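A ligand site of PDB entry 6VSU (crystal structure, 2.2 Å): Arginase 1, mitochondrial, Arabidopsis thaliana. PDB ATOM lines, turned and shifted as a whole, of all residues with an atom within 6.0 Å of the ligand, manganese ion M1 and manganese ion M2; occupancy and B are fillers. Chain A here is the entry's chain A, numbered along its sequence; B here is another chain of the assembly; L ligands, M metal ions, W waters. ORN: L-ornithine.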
ATOM      1  N   SER A  56      21.619 -34.738  21.075  1.00  0.00           N
ATOM      2  CA  SER A  56      21.453 -34.220  22.459  1.00  0.00           C
ATOM      3  C   SER A  56      20.203 -34.849  23.100  1.00  0.00           C
ATOM      4  O   SER A  56      20.070 -34.780  24.351  1.00  0.00           O
ATOM      5  CB  SER A  56      21.364 -32.714  22.488  1.00  0.00           C
ATOM      6  OG  SER A  56      20.315 -32.270  21.632  1.00  0.00           O
ATOM      7  N   HIS A 140      23.103 -33.918  12.746  1.00  0.00           N
ATOM      8  CA  HIS A 140      23.613 -32.727  12.050  1.00  0.00           C
ATOM      9  C   HIS A 140      25.124 -32.591  12.264  1.00  0.00           C
ATOM     10  O   HIS A 140      25.733 -31.812  11.517  1.00  0.00           O
ATOM     11  CB  HIS A 140      22.823 -31.478  12.464  1.00  0.00           C
ATOM     12  CG  HIS A 140      22.630 -30.543  11.322  1.00  0.00           C
ATOM     13  ND1 HIS A 140      21.509 -29.777  11.201  1.00  0.00           N
ATOM     14  CD2 HIS A 140      23.390 -30.334  10.220  1.00  0.00           C
ATOM     15  CE1 HIS A 140      21.573 -29.085  10.091  1.00  0.00           C
ATOM     16  NE2 HIS A 140      22.734 -29.418   9.444  1.00  0.00           N
ATOM     17  N   HIS A 162      21.452 -23.143   4.840  1.00  0.00           N
ATOM     18  CA  HIS A 162      21.291 -24.049   5.996  1.00  0.00           C
ATOM     19  C   HIS A 162      19.837 -23.983   6.397  1.00  0.00           C
ATOM     20  O   HIS A 162      19.479 -22.972   7.012  1.00  0.00           O
ATOM     21  CB  HIS A 162      22.287 -23.640   7.101  1.00  0.00           C
ATOM     22  CG  HIS A 162      22.044 -24.334   8.397  1.00  0.00           C
ATOM     23  ND1 HIS A 162      22.407 -23.757   9.606  1.00  0.00           N
ATOM     24  CD2 HIS A 162      21.473 -25.515   8.672  1.00  0.00           C
ATOM     25  CE1 HIS A 162      22.039 -24.588  10.577  1.00  0.00           C
ATOM     26  NE2 HIS A 162      21.464 -25.663  10.030  1.00  0.00           N
ATOM     27  N   ASP A 164      16.934 -25.196   8.821  1.00  0.00           N
ATOM     28  CA  ASP A 164      16.881 -25.812  10.162  1.00  0.00           C
ATOM     29  C   ASP A 164      16.020 -24.956  11.090  1.00  0.00           C
ATOM     30  O   ASP A 164      16.034 -23.726  10.948  1.00  0.00           O
ATOM     31  CB  ASP A 164      18.309 -25.942  10.663  1.00  0.00           C
ATOM     32  CG  ASP A 164      18.533 -26.988  11.740  1.00  0.00           C
ATOM     33  OD1 ASP A 164      17.620 -27.213  12.562  1.00  0.00           O
ATOM     34  OD2 ASP A 164      19.617 -27.593  11.724  1.00  0.00           O
ATOM     35  N   ALA A 165      15.253 -25.583  11.987  1.00  0.00           N
ATOM     36  CA  ALA A 165      14.636 -24.899  13.138  1.00  0.00           C
ATOM     37  C   ALA A 165      15.706 -24.257  14.024  1.00  0.00           C
ATOM     38  O   ALA A 165      15.392 -23.237  14.701  1.00  0.00           O
ATOM     39  CB  ALA A 165      13.802 -25.828  13.951  1.00  0.00           C
ATOM     40  N   HIS A 166      16.902 -24.857  14.048  1.00  0.00           N
ATOM     41  CA  HIS A 166      17.978 -24.518  15.021  1.00  0.00           C
ATOM     42  C   HIS A 166      19.217 -24.010  14.278  1.00  0.00           C
ATOM     43  O   HIS A 166      19.533 -24.469  13.184  1.00  0.00           O
ATOM     44  CB  HIS A 166      18.329 -25.784  15.851  1.00  0.00           C
ATOM     45  CG  HIS A 166      17.132 -26.526  16.391  1.00  0.00           C
ATOM     46  ND1 HIS A 166      16.538 -27.529  15.679  1.00  0.00           N
ATOM     47  CD2 HIS A 166      16.449 -26.398  17.570  1.00  0.00           C
ATOM     48  CE1 HIS A 166      15.507 -27.974  16.392  1.00  0.00           C
ATOM     49  NE2 HIS A 166      15.450 -27.302  17.565  1.00  0.00           N
ATOM     50  N   PRO A 167      20.012 -23.087  14.874  1.00  0.00           N
ATOM     51  CA  PRO A 167      21.199 -22.596  14.180  1.00  0.00           C
ATOM     52  C   PRO A 167      22.443 -23.513  14.285  1.00  0.00           C
ATOM     53  O   PRO A 167      23.335 -23.364  13.463  1.00  0.00           O
ATOM     54  CB  PRO A 167      21.404 -21.207  14.785  1.00  0.00           C
ATOM     55  CG  PRO A 167      20.780 -21.269  16.161  1.00  0.00           C
ATOM     56  CD  PRO A 167      19.758 -22.383  16.138  1.00  0.00           C
ATOM     57  N   ASP A 168      22.473 -24.435  15.258  1.00  0.00           N
ATOM     58  CA  ASP A 168      23.543 -25.459  15.424  1.00  0.00           C
ATOM     59  C   ASP A 168      24.907 -24.753  15.475  1.00  0.00           C
ATOM     60  O   ASP A 168      25.867 -25.164  14.811  1.00  0.00           O
ATOM     61  CB  ASP A 168      23.446 -26.536  14.336  1.00  0.00           C
ATOM     62  CG  ASP A 168      22.172 -27.362  14.441  1.00  0.00           C
ATOM     63  OD1 ASP A 168      21.495 -27.285  15.488  1.00  0.00           O
ATOM     64  OD2 ASP A 168      21.896 -28.116  13.473  1.00  0.00           O
ATOM     65  N   TYR A 170      26.169 -23.258  18.735  1.00  0.00           N
ATOM     66  CA  TYR A 170      26.757 -23.299  20.113  1.00  0.00           C
ATOM     67  C   TYR A 170      28.247 -23.624  20.053  1.00  0.00           C
ATOM     68  O   TYR A 170      28.716 -24.468  19.245  1.00  0.00           O
ATOM     69  CB  TYR A 170      26.168 -24.437  20.948  1.00  0.00           C
ATOM     70  CG  TYR A 170      24.748 -24.288  21.394  1.00  0.00           C
ATOM     71  CD1 TYR A 170      24.446 -23.605  22.553  1.00  0.00           C
ATOM     72  CD2 TYR A 170      23.723 -24.825  20.660  1.00  0.00           C
ATOM     73  CE1 TYR A 170      23.135 -23.500  22.998  1.00  0.00           C
ATOM     74  CE2 TYR A 170      22.397 -24.684  21.072  1.00  0.00           C
ATOM     75  CZ  TYR A 170      22.107 -24.029  22.253  1.00  0.00           C
ATOM     76  OH  TYR A 170      20.827 -23.917  22.658  1.00  0.00           O
ATOM     77  N   PHE A 173      28.290 -27.717  22.711  1.00  0.00           N
ATOM     78  CA  PHE A 173      27.016 -28.097  23.356  1.00  0.00           C
ATOM     79  C   PHE A 173      27.294 -29.265  24.283  1.00  0.00           C
ATOM     80  O   PHE A 173      27.796 -30.281  23.770  1.00  0.00           O
ATOM     81  CB  PHE A 173      25.901 -28.386  22.342  1.00  0.00           C
ATOM     82  CG  PHE A 173      24.544 -28.441  22.984  1.00  0.00           C
ATOM     83  CD1 PHE A 173      23.940 -27.285  23.472  1.00  0.00           C
ATOM     84  CD2 PHE A 173      23.885 -29.640  23.134  1.00  0.00           C
ATOM     85  CE1 PHE A 173      22.682 -27.335  24.052  1.00  0.00           C
ATOM     86  CE2 PHE A 173      22.615 -29.693  23.707  1.00  0.00           C
ATOM     87  CZ  PHE A 173      22.014 -28.533  24.162  1.00  0.00           C
ATOM     88  N   HIS A 180      25.771 -32.242  17.492  1.00  0.00           N
ATOM     89  CA  HIS A 180      24.930 -31.862  16.328  1.00  0.00           C
ATOM     90  C   HIS A 180      24.482 -30.389  16.445  1.00  0.00           C
ATOM     91  O   HIS A 180      23.941 -29.854  15.459  1.00  0.00           O
ATOM     92  CB  HIS A 180      23.734 -32.817  16.210  1.00  0.00           C
ATOM     93  CG  HIS A 180      22.675 -32.727  17.251  1.00  0.00           C
ATOM     94  ND1 HIS A 180      21.407 -33.256  17.025  1.00  0.00           N
ATOM     95  CD2 HIS A 180      22.640 -32.236  18.498  1.00  0.00           C
ATOM     96  CE1 HIS A 180      20.641 -33.070  18.093  1.00  0.00           C
ATOM     97  NE2 HIS A 180      21.358 -32.437  18.994  1.00  0.00           N
ATOM     98  N   ALA A 181      24.629 -29.781  17.627  1.00  0.00           N
ATOM     99  CA  ALA A 181      24.213 -28.405  17.897  1.00  0.00           C
ATOM    100  C   ALA A 181      25.418 -27.480  17.774  1.00  0.00           C
ATOM    101  O   ALA A 181      25.238 -26.340  18.148  1.00  0.00           O
ATOM    102  CB  ALA A 181      23.591 -28.306  19.265  1.00  0.00           C
ATOM    103  N   PHE A 184      27.871 -25.964  12.887  1.00  0.00           N
ATOM    104  CA  PHE A 184      27.998 -24.692  12.133  1.00  0.00           C
ATOM    105  C   PHE A 184      29.028 -23.777  12.810  1.00  0.00           C
ATOM    106  O   PHE A 184      29.684 -23.051  12.084  1.00  0.00           O
ATOM    107  CB  PHE A 184      26.609 -24.132  11.836  1.00  0.00           C
ATOM    108  CG  PHE A 184      25.955 -24.950  10.757  1.00  0.00           C
ATOM    109  CD1 PHE A 184      26.263 -24.741   9.418  1.00  0.00           C
ATOM    110  CD2 PHE A 184      25.150 -26.024  11.079  1.00  0.00           C
ATOM    111  CE1 PHE A 184      25.720 -25.544   8.429  1.00  0.00           C
ATOM    112  CE2 PHE A 184      24.589 -26.812  10.098  1.00  0.00           C
ATOM    113  CZ  PHE A 184      24.875 -26.574   8.766  1.00  0.00           C
ATOM    114  N   SER A 203      14.020 -21.728  17.114  1.00  0.00           N
ATOM    115  CA  SER A 203      14.553 -22.182  18.427  1.00  0.00           C
ATOM    116  C   SER A 203      15.992 -21.746  18.494  1.00  0.00           C
ATOM    117  O   SER A 203      16.822 -22.440  17.919  1.00  0.00           O
ATOM    118  CB  SER A 203      14.446 -23.691  18.597  1.00  0.00           C
ATOM    119  OG  SER A 203      14.964 -24.083  19.851  1.00  0.00           O
ATOM    120  N   ASN A 205      18.689 -19.076  21.149  1.00  0.00           N
ATOM    121  CA  ASN A 205      18.867 -18.370  22.438  1.00  0.00           C
ATOM    122  C   ASN A 205      19.922 -17.266  22.252  1.00  0.00           C
ATOM    123  O   ASN A 205      20.354 -17.026  21.097  1.00  0.00           O
ATOM    124  CB  ASN A 205      19.190 -19.357  23.577  1.00  0.00           C
ATOM    125  CG  ASN A 205      20.530 -20.082  23.499  1.00  0.00           C
ATOM    126  OD1 ASN A 205      21.283 -19.966  22.531  1.00  0.00           O
ATOM    127  ND2 ASN A 205      20.817 -20.872  24.525  1.00  0.00           N
ATOM    128  N   ASP A 249      18.156 -29.780   7.523  1.00  0.00           N
ATOM    129  CA  ASP A 249      17.606 -30.440   8.742  1.00  0.00           C
ATOM    130  C   ASP A 249      16.100 -30.576   8.483  1.00  0.00           C
ATOM    131  O   ASP A 249      15.388 -29.538   8.330  1.00  0.00           O
ATOM    132  CB  ASP A 249      17.906 -29.634  10.000  1.00  0.00           C
ATOM    133  CG  ASP A 249      17.480 -30.297  11.311  1.00  0.00           C
ATOM    134  OD1 ASP A 249      16.469 -31.074  11.280  1.00  0.00           O
ATOM    135  OD2 ASP A 249      18.126 -29.968  12.339  1.00  0.00           O
ATOM    136  N   ASP A 251      13.846 -30.929  10.384  1.00  0.00           N
ATOM    137  CA  ASP A 251      13.027 -30.098  11.327  1.00  0.00           C
ATOM    138  C   ASP A 251      12.914 -28.634  10.845  1.00  0.00           C
ATOM    139  O   ASP A 251      12.294 -27.792  11.593  1.00  0.00           O
ATOM    140  CB  ASP A 251      13.514 -30.222  12.778  1.00  0.00           C
ATOM    141  CG  ASP A 251      14.830 -29.556  13.097  1.00  0.00           C
ATOM    142  OD1 ASP A 251      15.192 -28.563  12.410  1.00  0.00           O
ATOM    143  OD2 ASP A 251      15.541 -30.097  14.008  1.00  0.00           O
ATOM    144  N   CYS A 252      13.415 -28.288   9.642  1.00  0.00           N
ATOM    145  CA  CYS A 252      13.109 -26.970   9.042  1.00  0.00           C
ATOM    146  C   CYS A 252      11.612 -26.904   8.757  1.00  0.00           C
ATOM    147  O   CYS A 252      11.052 -25.790   8.818  1.00  0.00           O
ATOM    148  CB  CYS A 252      13.928 -26.627   7.802  1.00  0.00           C
ATOM    149  SG  CYS A 252      13.529 -27.603   6.330  1.00  0.00           S
ATOM    150  N   HIS A 263      13.618 -33.228  17.477  1.00  0.00           N
ATOM    151  CA  HIS A 263      13.210 -31.920  18.050  1.00  0.00           C
ATOM    152  C   HIS A 263      11.932 -31.387  17.403  1.00  0.00           C
ATOM    153  O   HIS A 263      12.031 -30.666  16.415  1.00  0.00           O
ATOM    154  CB  HIS A 263      14.384 -30.982  17.902  1.00  0.00           C
ATOM    155  CG  HIS A 263      15.577 -31.544  18.599  1.00  0.00           C
ATOM    156  ND1 HIS A 263      15.866 -31.254  19.903  1.00  0.00           N
ATOM    157  CD2 HIS A 263      16.526 -32.407  18.156  1.00  0.00           C
ATOM    158  CE1 HIS A 263      16.940 -31.935  20.261  1.00  0.00           C
ATOM    159  NE2 HIS A 263      17.367 -32.675  19.201  1.00  0.00           N
ATOM    160  N   VAL A 291      19.518 -34.351   6.769  1.00  0.00           N
ATOM    161  CA  VAL A 291      19.969 -34.902   8.078  1.00  0.00           C
ATOM    162  C   VAL A 291      18.798 -34.821   9.043  1.00  0.00           C
ATOM    163  O   VAL A 291      17.819 -34.156   8.733  1.00  0.00           O
ATOM    164  CB  VAL A 291      21.184 -34.157   8.639  1.00  0.00           C
ATOM    165  CG1 VAL A 291      22.343 -34.105   7.661  1.00  0.00           C
ATOM    166  CG2 VAL A 291      20.812 -32.752   9.072  1.00  0.00           C
ATOM    167  N   GLU A 292      18.922 -35.521  10.160  1.00  0.00           N
ATOM    168  CA  GLU A 292      18.024 -35.442  11.347  1.00  0.00           C
ATOM    169  C   GLU A 292      16.638 -36.025  11.086  1.00  0.00           C
ATOM    170  O   GLU A 292      15.748 -35.779  11.890  1.00  0.00           O
ATOM    171  CB  GLU A 292      17.907 -34.014  11.857  1.00  0.00           C
ATOM    172  CG  GLU A 292      19.168 -33.532  12.491  1.00  0.00           C
ATOM    173  CD  GLU A 292      19.586 -34.127  13.817  1.00  0.00           C
ATOM    174  OE1 GLU A 292      18.783 -34.876  14.406  1.00  0.00           O
ATOM    175  OE2 GLU A 292      20.749 -33.832  14.244  1.00  0.00           O
ATOM    176  N   GLY B  75      13.569 -31.673  27.433  1.00  0.00           N
ATOM    177  CA  GLY B  75      15.017 -31.560  27.108  1.00  0.00           C
ATOM    178  C   GLY B  75      15.303 -31.418  25.617  1.00  0.00           C
ATOM    179  O   GLY B  75      16.386 -31.072  25.270  1.00  0.00           O
ATOM    180  N   SER B  76      14.333 -31.614  24.724  1.00  0.00           N
ATOM    181  CA  SER B  76      14.521 -31.419  23.254  1.00  0.00           C
ATOM    182  C   SER B  76      14.472 -29.913  22.938  1.00  0.00           C
ATOM    183  O   SER B  76      14.934 -29.547  21.839  1.00  0.00           O
ATOM    184  CB  SER B  76      13.487 -32.194  22.452  1.00  0.00           C
ATOM    185  OG  SER B  76      12.214 -31.632  22.646  1.00  0.00           O
ATOM    186  N   THR B  77      13.985 -29.098  23.881  1.00  0.00           N
ATOM    187  CA  THR B  77      13.709 -27.659  23.704  1.00  0.00           C
ATOM    188  C   THR B  77      14.760 -26.808  24.420  1.00  0.00           C
ATOM    189  O   THR B  77      15.371 -27.285  25.379  1.00  0.00           O
ATOM    190  CB  THR B  77      12.305 -27.259  24.189  1.00  0.00           C
ATOM    191  OG1 THR B  77      12.096 -27.508  25.595  1.00  0.00           O
ATOM    192  CG2 THR B  77      11.247 -27.968  23.395  1.00  0.00           C
ATOM    193  N   ASN B  78      14.887 -25.552  24.076  1.00  0.00           N
ATOM    194  CA  ASN B  78      15.609 -24.642  25.019  1.00  0.00           C
ATOM    195  C   ASN B  78      14.572 -23.768  25.689  1.00  0.00           C
ATOM    196  O   ASN B  78      13.408 -23.839  25.272  1.00  0.00           O
ATOM    197  CB  ASN B  78      16.785 -23.890  24.387  1.00  0.00           C
ATOM    198  CG  ASN B  78      16.349 -22.958  23.300  1.00  0.00           C
ATOM    199  OD1 ASN B  78      15.381 -22.249  23.507  1.00  0.00           O
ATOM    200  ND2 ASN B  78      17.049 -22.936  22.189  1.00  0.00           N
HETATM  201  N   ORN L   1      17.976 -28.125  22.578  1.00  0.00           N
HETATM  202  CA  ORN L   1      18.987 -27.874  21.498  1.00  0.00           C
HETATM  203  CB  ORN L   1      18.568 -28.581  20.193  1.00  0.00           C
HETATM  204  CG  ORN L   1      19.666 -28.743  19.162  1.00  0.00           C
HETATM  205  CD  ORN L   1      19.198 -29.459  17.911  1.00  0.00           C
HETATM  206  NE  ORN L   1      20.226 -29.777  16.911  1.00  0.00           N
HETATM  207  C   ORN L   1      19.105 -26.355  21.278  1.00  0.00           C
HETATM  208  O   ORN L   1      19.280 -25.900  20.143  1.00  0.00           O
HETATM  209  OXT ORN L   1      19.029 -25.551  22.221  1.00  0.00           O
HETATM  210 MN    MN M   1      20.276 -28.991  12.968  1.00  0.00          MN
HETATM  211 MN    MN M   2      17.192 -28.750  13.837  1.00  0.00          MN
HETATM  212  O   HOH W   1      18.775 -23.307  19.522  1.00  0.00           O
HETATM  213  O   HOH W   2      21.055 -25.158  17.814  1.00  0.00           O
HETATM  214  O   HOH W   3      18.715 -27.365  24.976  1.00  0.00           O
HETATM  215  O   HOH W   4      18.238 -31.165  15.285  1.00  0.00           O
HETATM  216  O   HOH W   5      18.381 -30.893  22.946  1.00  0.00           O
HETATM  217  O   HOH W   6      18.880 -28.836  14.909  1.00  0.00           O
HETATM  218  O   HOH W   7      15.852 -26.868  21.120  1.00  0.00           O
HETATM  219  O   HOH W   8      21.201 -30.285  14.734  1.00  0.00           O
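Along chain A the residues within 4 Å of manganese ion M2 span positions 164 to 251.
Along chain A the residues within 4 Å of manganese ion M1 span positions 140 to 249. The nearest printed residue that does not touch manganese ion M1 is His 180 (4.5 Å).
The backbone NH of Phe 184 lies within hydrogen-bond range of the backbone carbonyl oxygen of Asp 168 (2.9 Å). OD2 of Asp 164 sits close to NE2 of His 162 (3.2 Å). The side-chain carboxylate (OD1) of Asp 251 lies close to the backbone NH (N) of Ala 165, 3.0 Å away. The backbone carbonyl oxygen (O) of Asp 249 sits close to the side-chain sulfur (SG) of Cys 252 (3.3 Å). O of Ala 181 is in hydrogen-bond range of N of Tyr 170, 3.3 Å away. The side-chain hydroxyl of Ser 203 sits at hydrogen-bond distance from the side-chain amide nitrogen of Asn 78 of chain B (3.3 Å). The backbone carbonyl oxygen (O) of Ser 76 of chain B is in hydrogen-bond range of a ring nitrogen (ND1) of His 263 (2.7 Å). NE2 of His 180 is in hydrogen-bond range of OG of Ser 56, at 2.8 Å.
Residues that only touch the ligand: His 180, His 263, Thr 77 of chain B and Ala 181. Hydrophobic or aromatic side chains within 4 Å of the ligand: His 166, Tyr 170, His 180, Ala 181 and His 263. The nearest printed residue that does not touch the ligand is Phe 173 (4.1 Å).
Water W6 lies within hydrogen-bond range of NE of the ligand (2.6 Å) and OD1 of Asp 168 (3.1 Å). Water W3 bridges N of the ligand (2.6 Å) and O of Thr 77 of chain B (3.4 Å). Water W1 lies within hydrogen-bond range of the backbone carbonyl oxygen of Ser 203 (2.7 Å), an oxygen (O) of the ligand (2.7 Å) and the side-chain amide nitrogen of Asn 78 of chain B (3.2 Å). Water W5 lies within hydrogen-bond range of OG of Ser 56 (2.7 Å), N of the ligand (2.8 Å) and O of Gly 75 of chain B (3.1 Å). Water W7 lies within hydrogen-bond range of N of the ligand (2.9 Å), O of Ser 76 of chain B (2.9 Å), OG of Ser 203 (3.2 Å) and N of Asn 78 of chain B (3.4 Å). Water W2 bridges the backbone NH of Asp 168 and an oxygen (O) of the ligand.
Manganese ion M1 is bound by the side-chain carboxylate (OD2) of Asp 168, the side-chain carboxylate (OD2) of Asp 164, a ring nitrogen (ND1) of His 140, water W8, water W6 and the side-chain carboxylate (OD2) of Asp 249.
The side-chain carboxylate of Asp 168 is in salt-bridge range of a nitrogen (NE) of the ligand (3.1 Å). OH of Tyr 170 sits at hydrogen-bond distance from OXT of the ligand. The side-chain amide nitrogen of Asn 78 of chain B is in hydrogen-bond range of an oxygen (OXT) of the ligand (3.3 Å). A nitrogen (N) of the ligand is in hydrogen-bond range of the backbone carbonyl oxygen (O) of Ser 76 of chain B.
Manganese ion M2 is bound by water W6 (2.0 Å), OD1 of Asp 164 (2.0 Å), OD2 of Asp 251 (2.1 Å), OD2 of Asp 249 (2.1 Å), ND1 of His 166 (2.3 Å) and OD1 of Asp 251 (2.5 Å).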
